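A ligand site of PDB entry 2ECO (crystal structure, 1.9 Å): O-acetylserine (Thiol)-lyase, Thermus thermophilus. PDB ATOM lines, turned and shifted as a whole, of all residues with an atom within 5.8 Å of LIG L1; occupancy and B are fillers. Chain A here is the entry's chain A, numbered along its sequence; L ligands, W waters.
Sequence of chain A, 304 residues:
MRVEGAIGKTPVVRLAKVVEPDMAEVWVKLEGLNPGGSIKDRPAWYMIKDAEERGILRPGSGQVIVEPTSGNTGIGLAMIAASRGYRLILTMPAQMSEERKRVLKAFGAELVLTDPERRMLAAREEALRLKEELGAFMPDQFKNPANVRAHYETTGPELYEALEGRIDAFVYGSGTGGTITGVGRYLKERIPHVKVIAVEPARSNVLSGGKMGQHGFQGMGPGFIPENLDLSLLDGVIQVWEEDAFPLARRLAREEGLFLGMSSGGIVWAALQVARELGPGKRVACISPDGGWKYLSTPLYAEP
Merely in contact with LIG L1: Gly 219, Gln 218, Pro 289, Gly 173, Asp 290, Gly 178, Ser 174 and Met 220.
Water W3 lies within hydrogen-bond range of O5 of LIG L1 (2.6 Å), N of Ile 180 (3.0 Å) and OG of Ser 174 (3.1 Å). Water W4 lies within hydrogen-bond range of a ring nitrogen (NE2) of His 151 (2.7 Å), an oxygen (O4) of LIG L1 (2.7 Å) and the side-chain amide oxygen of Asn 147 (2.8 Å). Water W2 lies within hydrogen-bond range of N of Asn 72 (2.9 Å), O1 of LIG L1 (3.1 Å) and O2 of LG2 L2 (3.1 Å). Water W1 lies within hydrogen-bond range of O of Gln 218 (2.7 Å), N of Ser 263 (2.9 Å) and OH of Tyr 295 (3.3 Å).
The side-chain hydroxyl of Ser 38 lies close to the backbone NH of Lys 40. The side-chain hydroxyl (OG1) of Thr 179 lies within hydrogen-bond range of a ring nitrogen (NE2) of His 151, 3.2 Å away. N of Gly 178 is in hydrogen-bond range of OG1 of Thr 176, at 3.2 Å. ND2 of Asn 147 lies within hydrogen-bond range of OG1 of Thr 176, at 3.0 Å. OD1 of Asp 290 is in hydrogen-bond range of ND2 of Asn 72 (3.0 Å). The backbone carbonyl oxygen (O) of Pro 289 is in hydrogen-bond range of the backbone NH (N) of Ile 39. OD1 of Asp 290 is in hydrogen-bond range of OH of Tyr 295, at 2.5 Å.
A carbon (C5) of LIG L1 is bonded to the side-chain amino group of Lys 40 (1.4 Å). The side-chain hydroxyl of Tyr 172 sits at hydrogen-bond distance from an oxygen (O2) of LIG L1 (2.6 Å). The backbone NH (N) of Thr 179 is in hydrogen-bond range of an oxygen (O4) of LIG L1 (2.9 Å). O4 of LIG L1 lies within hydrogen-bond range of OG1 of Thr 179 (2.6 Å). N of Thr 176 lies within hydrogen-bond range of O3 of LIG L1, 2.8 Å away. The side-chain hydroxyl (OG1) of Thr 176 lies within hydrogen-bond range of an oxygen (O3) of LIG L1 (2.7 Å). O1 of LIG L1 is in hydrogen-bond range of ND2 of Asn 72. O5 of LIG L1 lies within hydrogen-bond range of N of Gly 175 (2.8 Å). The side-chain hydroxyl (OG) of Ser 263 lies within hydrogen-bond range of a nitrogen (N1) of LIG L1, 2.8 Å away. N of Gly 177 is in hydrogen-bond range of O5 of LIG L1 (3.1 Å). The side-chain amino group (NZ) of Lys 40 is in salt-bridge range of an oxygen (O2) of LG2 L2 (3.7 Å). O2 of LG2 L2 sits at hydrogen-bond distance from N of Asn 72 (3.2 Å). The backbone NH (N) of Thr 73 lies within hydrogen-bond range of an oxygen (O2) of LG2 L2, at 3.1 Å. An oxygen (O2) of LG2 L2 sits at hydrogen-bond distance from the side-chain hydroxyl (OG1) of Thr 73 (3.3 Å). An oxygen (O1) of LG2 L2 lies within hydrogen-bond range of the side-chain amide nitrogen (NE2) of Gln 141 (3.3 Å).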
ATOM      1  N   SER A  38      -9.142  10.075 -22.534  1.00  0.00           N
ATOM      2  CA  SER A  38      -7.727   9.720 -22.375  1.00  0.00           C
ATOM      3  C   SER A  38      -7.364   9.274 -20.967  1.00  0.00           C
ATOM      4  O   SER A  38      -8.157   9.391 -20.033  1.00  0.00           O
ATOM      5  CB  SER A  38      -6.830  10.901 -22.730  1.00  0.00           C
ATOM      6  OG  SER A  38      -6.698  11.787 -21.620  1.00  0.00           O
ATOM      7  N   ILE A  39      -6.141   8.795 -20.828  1.00  0.00           N
ATOM      8  CA  ILE A  39      -5.615   8.339 -19.554  1.00  0.00           C
ATOM      9  C   ILE A  39      -5.577   9.475 -18.522  1.00  0.00           C
ATOM     10  O   ILE A  39      -5.577   9.211 -17.315  1.00  0.00           O
ATOM     11  CB  ILE A  39      -4.189   7.753 -19.732  1.00  0.00           C
ATOM     12  CG1 ILE A  39      -3.709   7.123 -18.437  1.00  0.00           C
ATOM     13  CG2 ILE A  39      -3.246   8.838 -20.218  1.00  0.00           C
ATOM     14  CD1 ILE A  39      -2.378   6.410 -18.585  1.00  0.00           C
ATOM     15  N   LYS A  40      -5.546  10.720 -18.993  1.00  0.00           N
ATOM     16  CA  LYS A  40      -5.495  11.867 -18.078  1.00  0.00           C
ATOM     17  C   LYS A  40      -6.720  12.011 -17.181  1.00  0.00           C
ATOM     18  O   LYS A  40      -6.705  12.785 -16.227  1.00  0.00           O
ATOM     19  CB  LYS A  40      -5.295  13.172 -18.833  1.00  0.00           C
ATOM     20  CG  LYS A  40      -3.927  13.344 -19.453  1.00  0.00           C
ATOM     21  CD  LYS A  40      -2.796  13.196 -18.420  1.00  0.00           C
ATOM     22  CE  LYS A  40      -1.512  13.861 -18.922  1.00  0.00           C
ATOM     23  NZ  LYS A  40      -1.264  13.464 -20.329  1.00  0.00           N
ATOM     24  N   ASN A  72      -4.621  16.732 -22.962  1.00  0.00           N
ATOM     25  CA  ASN A  72      -5.574  15.831 -22.336  1.00  0.00           C
ATOM     26  C   ASN A  72      -5.824  16.160 -20.863  1.00  0.00           C
ATOM     27  O   ASN A  72      -6.930  15.956 -20.367  1.00  0.00           O
ATOM     28  CB  ASN A  72      -5.101  14.377 -22.471  1.00  0.00           C
ATOM     29  CG  ASN A  72      -5.343  13.822 -23.860  1.00  0.00           C
ATOM     30  OD1 ASN A  72      -6.355  14.129 -24.499  1.00  0.00           O
ATOM     31  ND2 ASN A  72      -4.425  12.998 -24.339  1.00  0.00           N
ATOM     32  N   THR A  73      -4.822  16.673 -20.172  1.00  0.00           N
ATOM     33  CA  THR A  73      -5.009  17.024 -18.764  1.00  0.00           C
ATOM     34  C   THR A  73      -6.045  18.147 -18.668  1.00  0.00           C
ATOM     35  O   THR A  73      -6.886  18.139 -17.774  1.00  0.00           O
ATOM     36  CB  THR A  73      -3.685  17.474 -18.126  1.00  0.00           C
ATOM     37  OG1 THR A  73      -2.771  16.372 -18.127  1.00  0.00           O
ATOM     38  CG2 THR A  73      -3.904  17.925 -16.682  1.00  0.00           C
ATOM     39  N   GLN A 141       0.339  19.284 -12.388  1.00  0.00           N
ATOM     40  CA  GLN A 141       0.471  17.915 -12.883  1.00  0.00           C
ATOM     41  C   GLN A 141       1.859  17.271 -12.950  1.00  0.00           C
ATOM     42  O   GLN A 141       1.975  16.058 -12.805  1.00  0.00           O
ATOM     43  CB  GLN A 141      -0.193  17.790 -14.257  1.00  0.00           C
ATOM     44  CG  GLN A 141       0.567  18.449 -15.394  1.00  0.00           C
ATOM     45  CD  GLN A 141      -0.055  18.127 -16.744  1.00  0.00           C
ATOM     46  OE1 GLN A 141      -0.534  17.023 -16.958  1.00  0.00           O
ATOM     47  NE2 GLN A 141      -0.036  19.090 -17.662  1.00  0.00           N
ATOM     48  N   ASN A 147      -0.975  12.441  -8.815  1.00  0.00           N
ATOM     49  CA  ASN A 147      -0.948  12.037 -10.220  1.00  0.00           C
ATOM     50  C   ASN A 147      -0.431  10.590 -10.229  1.00  0.00           C
ATOM     51  O   ASN A 147      -1.089   9.677 -10.724  1.00  0.00           O
ATOM     52  CB  ASN A 147       0.007  12.953 -11.004  1.00  0.00           C
ATOM     53  CG  ASN A 147       0.139  12.570 -12.470  1.00  0.00           C
ATOM     54  OD1 ASN A 147      -0.085  11.424 -12.856  1.00  0.00           O
ATOM     55  ND2 ASN A 147       0.544  13.543 -13.290  1.00  0.00           N
ATOM     56  N   HIS A 151      -2.297   6.147 -10.696  1.00  0.00           N
ATOM     57  CA  HIS A 151      -1.853   4.968 -11.438  1.00  0.00           C
ATOM     58  C   HIS A 151      -1.389   3.836 -10.534  1.00  0.00           C
ATOM     59  O   HIS A 151      -1.526   2.655 -10.884  1.00  0.00           O
ATOM     60  CB  HIS A 151      -0.761   5.389 -12.419  1.00  0.00           C
ATOM     61  CG  HIS A 151      -1.222   6.440 -13.390  1.00  0.00           C
ATOM     62  ND1 HIS A 151      -2.179   6.179 -14.355  1.00  0.00           N
ATOM     63  CD2 HIS A 151      -0.922   7.756 -13.502  1.00  0.00           C
ATOM     64  CE1 HIS A 151      -2.449   7.298 -15.016  1.00  0.00           C
ATOM     65  NE2 HIS A 151      -1.692   8.262 -14.514  1.00  0.00           N
ATOM     66  N   TYR A 172       6.053   2.413 -21.738  1.00  0.00           N
ATOM     67  CA  TYR A 172       5.200   3.596 -21.773  1.00  0.00           C
ATOM     68  C   TYR A 172       5.900   4.881 -22.214  1.00  0.00           C
ATOM     69  O   TYR A 172       7.054   5.111 -21.878  1.00  0.00           O
ATOM     70  CB  TYR A 172       4.561   3.831 -20.401  1.00  0.00           C
ATOM     71  CG  TYR A 172       3.454   4.848 -20.428  1.00  0.00           C
ATOM     72  CD1 TYR A 172       2.249   4.567 -21.075  1.00  0.00           C
ATOM     73  CD2 TYR A 172       3.614   6.112 -19.840  1.00  0.00           C
ATOM     74  CE1 TYR A 172       1.223   5.511 -21.141  1.00  0.00           C
ATOM     75  CE2 TYR A 172       2.599   7.056 -19.896  1.00  0.00           C
ATOM     76  CZ  TYR A 172       1.409   6.758 -20.553  1.00  0.00           C
ATOM     77  OH  TYR A 172       0.398   7.686 -20.627  1.00  0.00           O
ATOM     78  N   GLY A 173       5.179   5.711 -22.968  1.00  0.00           N
ATOM     79  CA  GLY A 173       5.715   6.976 -23.444  1.00  0.00           C
ATOM     80  C   GLY A 173       5.406   8.016 -22.384  1.00  0.00           C
ATOM     81  O   GLY A 173       4.277   8.490 -22.267  1.00  0.00           O
ATOM     82  N   SER A 174       6.426   8.376 -21.602  1.00  0.00           N
ATOM     83  CA  SER A 174       6.260   9.315 -20.501  1.00  0.00           C
ATOM     84  C   SER A 174       5.986  10.769 -20.827  1.00  0.00           C
ATOM     85  O   SER A 174       6.600  11.353 -21.722  1.00  0.00           O
ATOM     86  CB  SER A 174       7.485   9.243 -19.579  1.00  0.00           C
ATOM     87  OG  SER A 174       7.229   9.888 -18.344  1.00  0.00           O
ATOM     88  N   GLY A 175       5.055  11.345 -20.069  1.00  0.00           N
ATOM     89  CA  GLY A 175       4.699  12.745 -20.218  1.00  0.00           C
ATOM     90  C   GLY A 175       4.976  13.406 -18.877  1.00  0.00           C
ATOM     91  O   GLY A 175       6.052  13.963 -18.678  1.00  0.00           O
ATOM     92  N   THR A 176       4.015  13.330 -17.953  1.00  0.00           N
ATOM     93  CA  THR A 176       4.204  13.898 -16.611  1.00  0.00           C
ATOM     94  C   THR A 176       5.021  12.928 -15.759  1.00  0.00           C
ATOM     95  O   THR A 176       5.579  13.306 -14.730  1.00  0.00           O
ATOM     96  CB  THR A 176       2.855  14.131 -15.869  1.00  0.00           C
ATOM     97  OG1 THR A 176       2.201  12.864 -15.665  1.00  0.00           O
ATOM     98  CG2 THR A 176       1.950  15.063 -16.659  1.00  0.00           C
ATOM     99  N   GLY A 177       5.085  11.673 -16.205  1.00  0.00           N
ATOM    100  CA  GLY A 177       5.820  10.668 -15.458  1.00  0.00           C
ATOM    101  C   GLY A 177       4.929   9.893 -14.506  1.00  0.00           C
ATOM    102  O   GLY A 177       5.342   8.872 -13.947  1.00  0.00           O
ATOM    103  N   GLY A 178       3.702  10.367 -14.314  1.00  0.00           N
ATOM    104  CA  GLY A 178       2.780   9.717 -13.403  1.00  0.00           C
ATOM    105  C   GLY A 178       2.467   8.249 -13.681  1.00  0.00           C
ATOM    106  O   GLY A 178       2.526   7.422 -12.771  1.00  0.00           O
ATOM    107  N   THR A 179       2.148   7.937 -14.932  1.00  0.00           N
ATOM    108  CA  THR A 179       1.800   6.568 -15.318  1.00  0.00           C
ATOM    109  C   THR A 179       2.932   5.559 -15.141  1.00  0.00           C
ATOM    110  O   THR A 179       2.756   4.529 -14.497  1.00  0.00           O
ATOM    111  CB  THR A 179       1.326   6.520 -16.785  1.00  0.00           C
ATOM    112  OG1 THR A 179       0.170   7.359 -16.945  1.00  0.00           O
ATOM    113  CG2 THR A 179       0.970   5.086 -17.187  1.00  0.00           C
ATOM    114  N   ILE A 180       4.085   5.847 -15.724  1.00  0.00           N
ATOM    115  CA  ILE A 180       5.187   4.909 -15.640  1.00  0.00           C
ATOM    116  C   ILE A 180       5.668   4.727 -14.198  1.00  0.00           C
ATOM    117  O   ILE A 180       6.056   3.631 -13.806  1.00  0.00           O
ATOM    118  CB  ILE A 180       6.343   5.321 -16.587  1.00  0.00           C
ATOM    119  CG1 ILE A 180       7.246   4.115 -16.864  1.00  0.00           C
ATOM    120  CG2 ILE A 180       7.137   6.470 -15.984  1.00  0.00           C
ATOM    121  CD1 ILE A 180       8.179   4.319 -18.037  1.00  0.00           C
ATOM    122  N   GLN A 218       1.984  14.112 -29.583  1.00  0.00           N
ATOM    123  CA  GLN A 218       1.223  14.896 -28.614  1.00  0.00           C
ATOM    124  C   GLN A 218       0.910  14.149 -27.327  1.00  0.00           C
ATOM    125  O   GLN A 218       0.450  13.013 -27.342  1.00  0.00           O
ATOM    126  CB  GLN A 218      -0.079  15.402 -29.262  1.00  0.00           C
ATOM    127  CG  GLN A 218       0.137  16.209 -30.536  1.00  0.00           C
ATOM    128  CD  GLN A 218      -1.131  16.901 -31.031  1.00  0.00           C
ATOM    129  OE1 GLN A 218      -1.205  17.300 -32.193  1.00  0.00           O
ATOM    130  NE2 GLN A 218      -2.106  17.052 -30.151  1.00  0.00           N
ATOM    131  N   GLY A 219       1.170  14.816 -26.200  1.00  0.00           N
ATOM    132  CA  GLY A 219       0.887  14.211 -24.905  1.00  0.00           C
ATOM    133  C   GLY A 219       2.075  13.612 -24.191  1.00  0.00           C
ATOM    134  O   GLY A 219       2.031  13.448 -22.968  1.00  0.00           O
ATOM    135  N   MET A 220       3.137  13.276 -24.913  1.00  0.00           N
ATOM    136  CA  MET A 220       4.336  12.707 -24.289  1.00  0.00           C
ATOM    137  C   MET A 220       5.576  13.488 -24.705  1.00  0.00           C
ATOM    138  O   MET A 220       5.508  14.319 -25.604  1.00  0.00           O
ATOM    139  CB  MET A 220       4.510  11.234 -24.686  1.00  0.00           C
ATOM    140  CG  MET A 220       4.729  10.984 -26.171  1.00  0.00           C
ATOM    141  SD  MET A 220       5.079   9.238 -26.549  1.00  0.00           S
ATOM    142  CE  MET A 220       6.837   9.202 -26.328  1.00  0.00           C
ATOM    143  N   SER A 263       0.776   9.398 -29.636  1.00  0.00           N
ATOM    144  CA  SER A 263       1.683   8.795 -28.665  1.00  0.00           C
ATOM    145  C   SER A 263       1.557   7.274 -28.650  1.00  0.00           C
ATOM    146  O   SER A 263       2.541   6.574 -28.401  1.00  0.00           O
ATOM    147  CB  SER A 263       1.432   9.372 -27.263  1.00  0.00           C
ATOM    148  OG  SER A 263       0.126   9.093 -26.804  1.00  0.00           O
ATOM    149  N   ILE A 267       4.545   4.473 -28.634  1.00  0.00           N
ATOM    150  CA  ILE A 267       4.586   3.518 -27.530  1.00  0.00           C
ATOM    151  C   ILE A 267       4.511   2.075 -28.022  1.00  0.00           C
ATOM    152  O   ILE A 267       5.293   1.227 -27.591  1.00  0.00           O
ATOM    153  CB  ILE A 267       3.436   3.792 -26.536  1.00  0.00           C
ATOM    154  CG1 ILE A 267       3.691   5.149 -25.857  1.00  0.00           C
ATOM    155  CG2 ILE A 267       3.340   2.665 -25.503  1.00  0.00           C
ATOM    156  CD1 ILE A 267       2.512   5.674 -25.044  1.00  0.00           C
ATOM    157  N   PRO A 289      -2.478   5.873 -24.519  1.00  0.00           N
ATOM    158  CA  PRO A 289      -2.996   7.061 -23.820  1.00  0.00           C
ATOM    159  C   PRO A 289      -4.357   7.559 -24.293  1.00  0.00           C
ATOM    160  O   PRO A 289      -5.194   7.932 -23.487  1.00  0.00           O
ATOM    161  CB  PRO A 289      -1.889   8.084 -24.029  1.00  0.00           C
ATOM    162  CG  PRO A 289      -0.649   7.209 -24.111  1.00  0.00           C
ATOM    163  CD  PRO A 289      -1.113   6.108 -25.008  1.00  0.00           C
ATOM    164  N   ASP A 290      -4.577   7.589 -25.607  1.00  0.00           N
ATOM    165  CA  ASP A 290      -5.857   8.021 -26.140  1.00  0.00           C
ATOM    166  C   ASP A 290      -6.104   7.494 -27.554  1.00  0.00           C
ATOM    167  O   ASP A 290      -5.211   6.880 -28.155  1.00  0.00           O
ATOM    168  CB  ASP A 290      -6.021   9.560 -26.077  1.00  0.00           C
ATOM    169  CG  ASP A 290      -4.997  10.329 -26.913  1.00  0.00           C
ATOM    170  OD1 ASP A 290      -5.067  11.582 -26.887  1.00  0.00           O
ATOM    171  OD2 ASP A 290      -4.153   9.718 -27.600  1.00  0.00           O
ATOM    172  N   TYR A 295      -7.087  13.452 -33.569  1.00  0.00           N
ATOM    173  CA  TYR A 295      -6.000  13.727 -34.500  1.00  0.00           C
ATOM    174  C   TYR A 295      -6.267  13.526 -35.987  1.00  0.00           C
ATOM    175  O   TYR A 295      -5.345  13.265 -36.766  1.00  0.00           O
ATOM    176  CB  TYR A 295      -4.774  12.902 -34.075  1.00  0.00           C
ATOM    177  CG  TYR A 295      -4.528  12.950 -32.585  1.00  0.00           C
ATOM    178  CD1 TYR A 295      -4.969  11.916 -31.748  1.00  0.00           C
ATOM    179  CD2 TYR A 295      -3.877  14.035 -32.000  1.00  0.00           C
ATOM    180  CE1 TYR A 295      -4.771  11.972 -30.366  1.00  0.00           C
ATOM    181  CE2 TYR A 295      -3.665  14.107 -30.623  1.00  0.00           C
ATOM    182  CZ  TYR A 295      -4.120  13.070 -29.814  1.00  0.00           C
ATOM    183  OH  TYR A 295      -3.909  13.140 -28.447  1.00  0.00           O
HETATM  184  N1  LIG L   1       0.282  10.469 -24.323  1.00  0.00           N
HETATM  185  C1  LIG L   1      -0.811  11.268 -24.226  1.00  0.00           C
HETATM  186  C2  LIG L   1      -1.686  11.511 -25.479  1.00  0.00           C
HETATM  187  C3  LIG L   1      -1.127  11.852 -23.001  1.00  0.00           C
HETATM  188  O1  LIG L   1      -2.216  12.664 -22.886  1.00  0.00           O
HETATM  189  C4  LIG L   1      -0.337  11.610 -21.880  1.00  0.00           C
HETATM  190  C5  LIG L   1      -0.700  12.247 -20.525  1.00  0.00           C
HETATM  191  C6  LIG L   1       0.791  10.789 -21.988  1.00  0.00           C
HETATM  192  C7  LIG L   1       1.081  10.222 -23.213  1.00  0.00           C
HETATM  193  C8  LIG L   1       1.755  10.469 -20.783  1.00  0.00           C
HETATM  194  O2  LIG L   1       1.192   9.917 -19.521  1.00  0.00           O
HETATM  195  P1  LIG L   1       1.865  10.507 -18.191  1.00  0.00           P
HETATM  196  O3  LIG L   1       1.555  11.957 -18.078  1.00  0.00           O
HETATM  197  O4  LIG L   1       1.258   9.739 -16.992  1.00  0.00           O
HETATM  198  O5  LIG L   1       3.308  10.142 -18.270  1.00  0.00           O
HETATM  199  C1  LG2 L   2       0.216  17.077 -20.248  1.00  0.00           C
HETATM  200  C2  LG2 L   2       1.333  16.926 -21.293  1.00  0.00           C
HETATM  201  C3  LG2 L   2       2.598  16.246 -20.749  1.00  0.00           C
HETATM  202  C4  LG2 L   2       2.206  14.860 -20.270  1.00  0.00           C
HETATM  203  C5  LG2 L   2       3.652  16.143 -21.835  1.00  0.00           C
HETATM  204  C6  LG2 L   2      -1.022  17.747 -20.805  1.00  0.00           C
HETATM  205  O1  LG2 L   2      -1.071  18.996 -20.771  1.00  0.00           O
HETATM  206  O2  LG2 L   2      -1.928  17.020 -21.271  1.00  0.00           O
HETATM  207  O   HOH W   1      -1.118  11.456 -28.844  1.00  0.00           O
HETATM  208  O   HOH W   2      -2.203  15.561 -24.007  1.00  0.00           O
HETATM  209  O   HOH W   3       4.753   8.200 -17.405  1.00  0.00           O
HETATM  210  O   HOH W   4      -0.779  10.654 -15.414  1.00  0.00           O
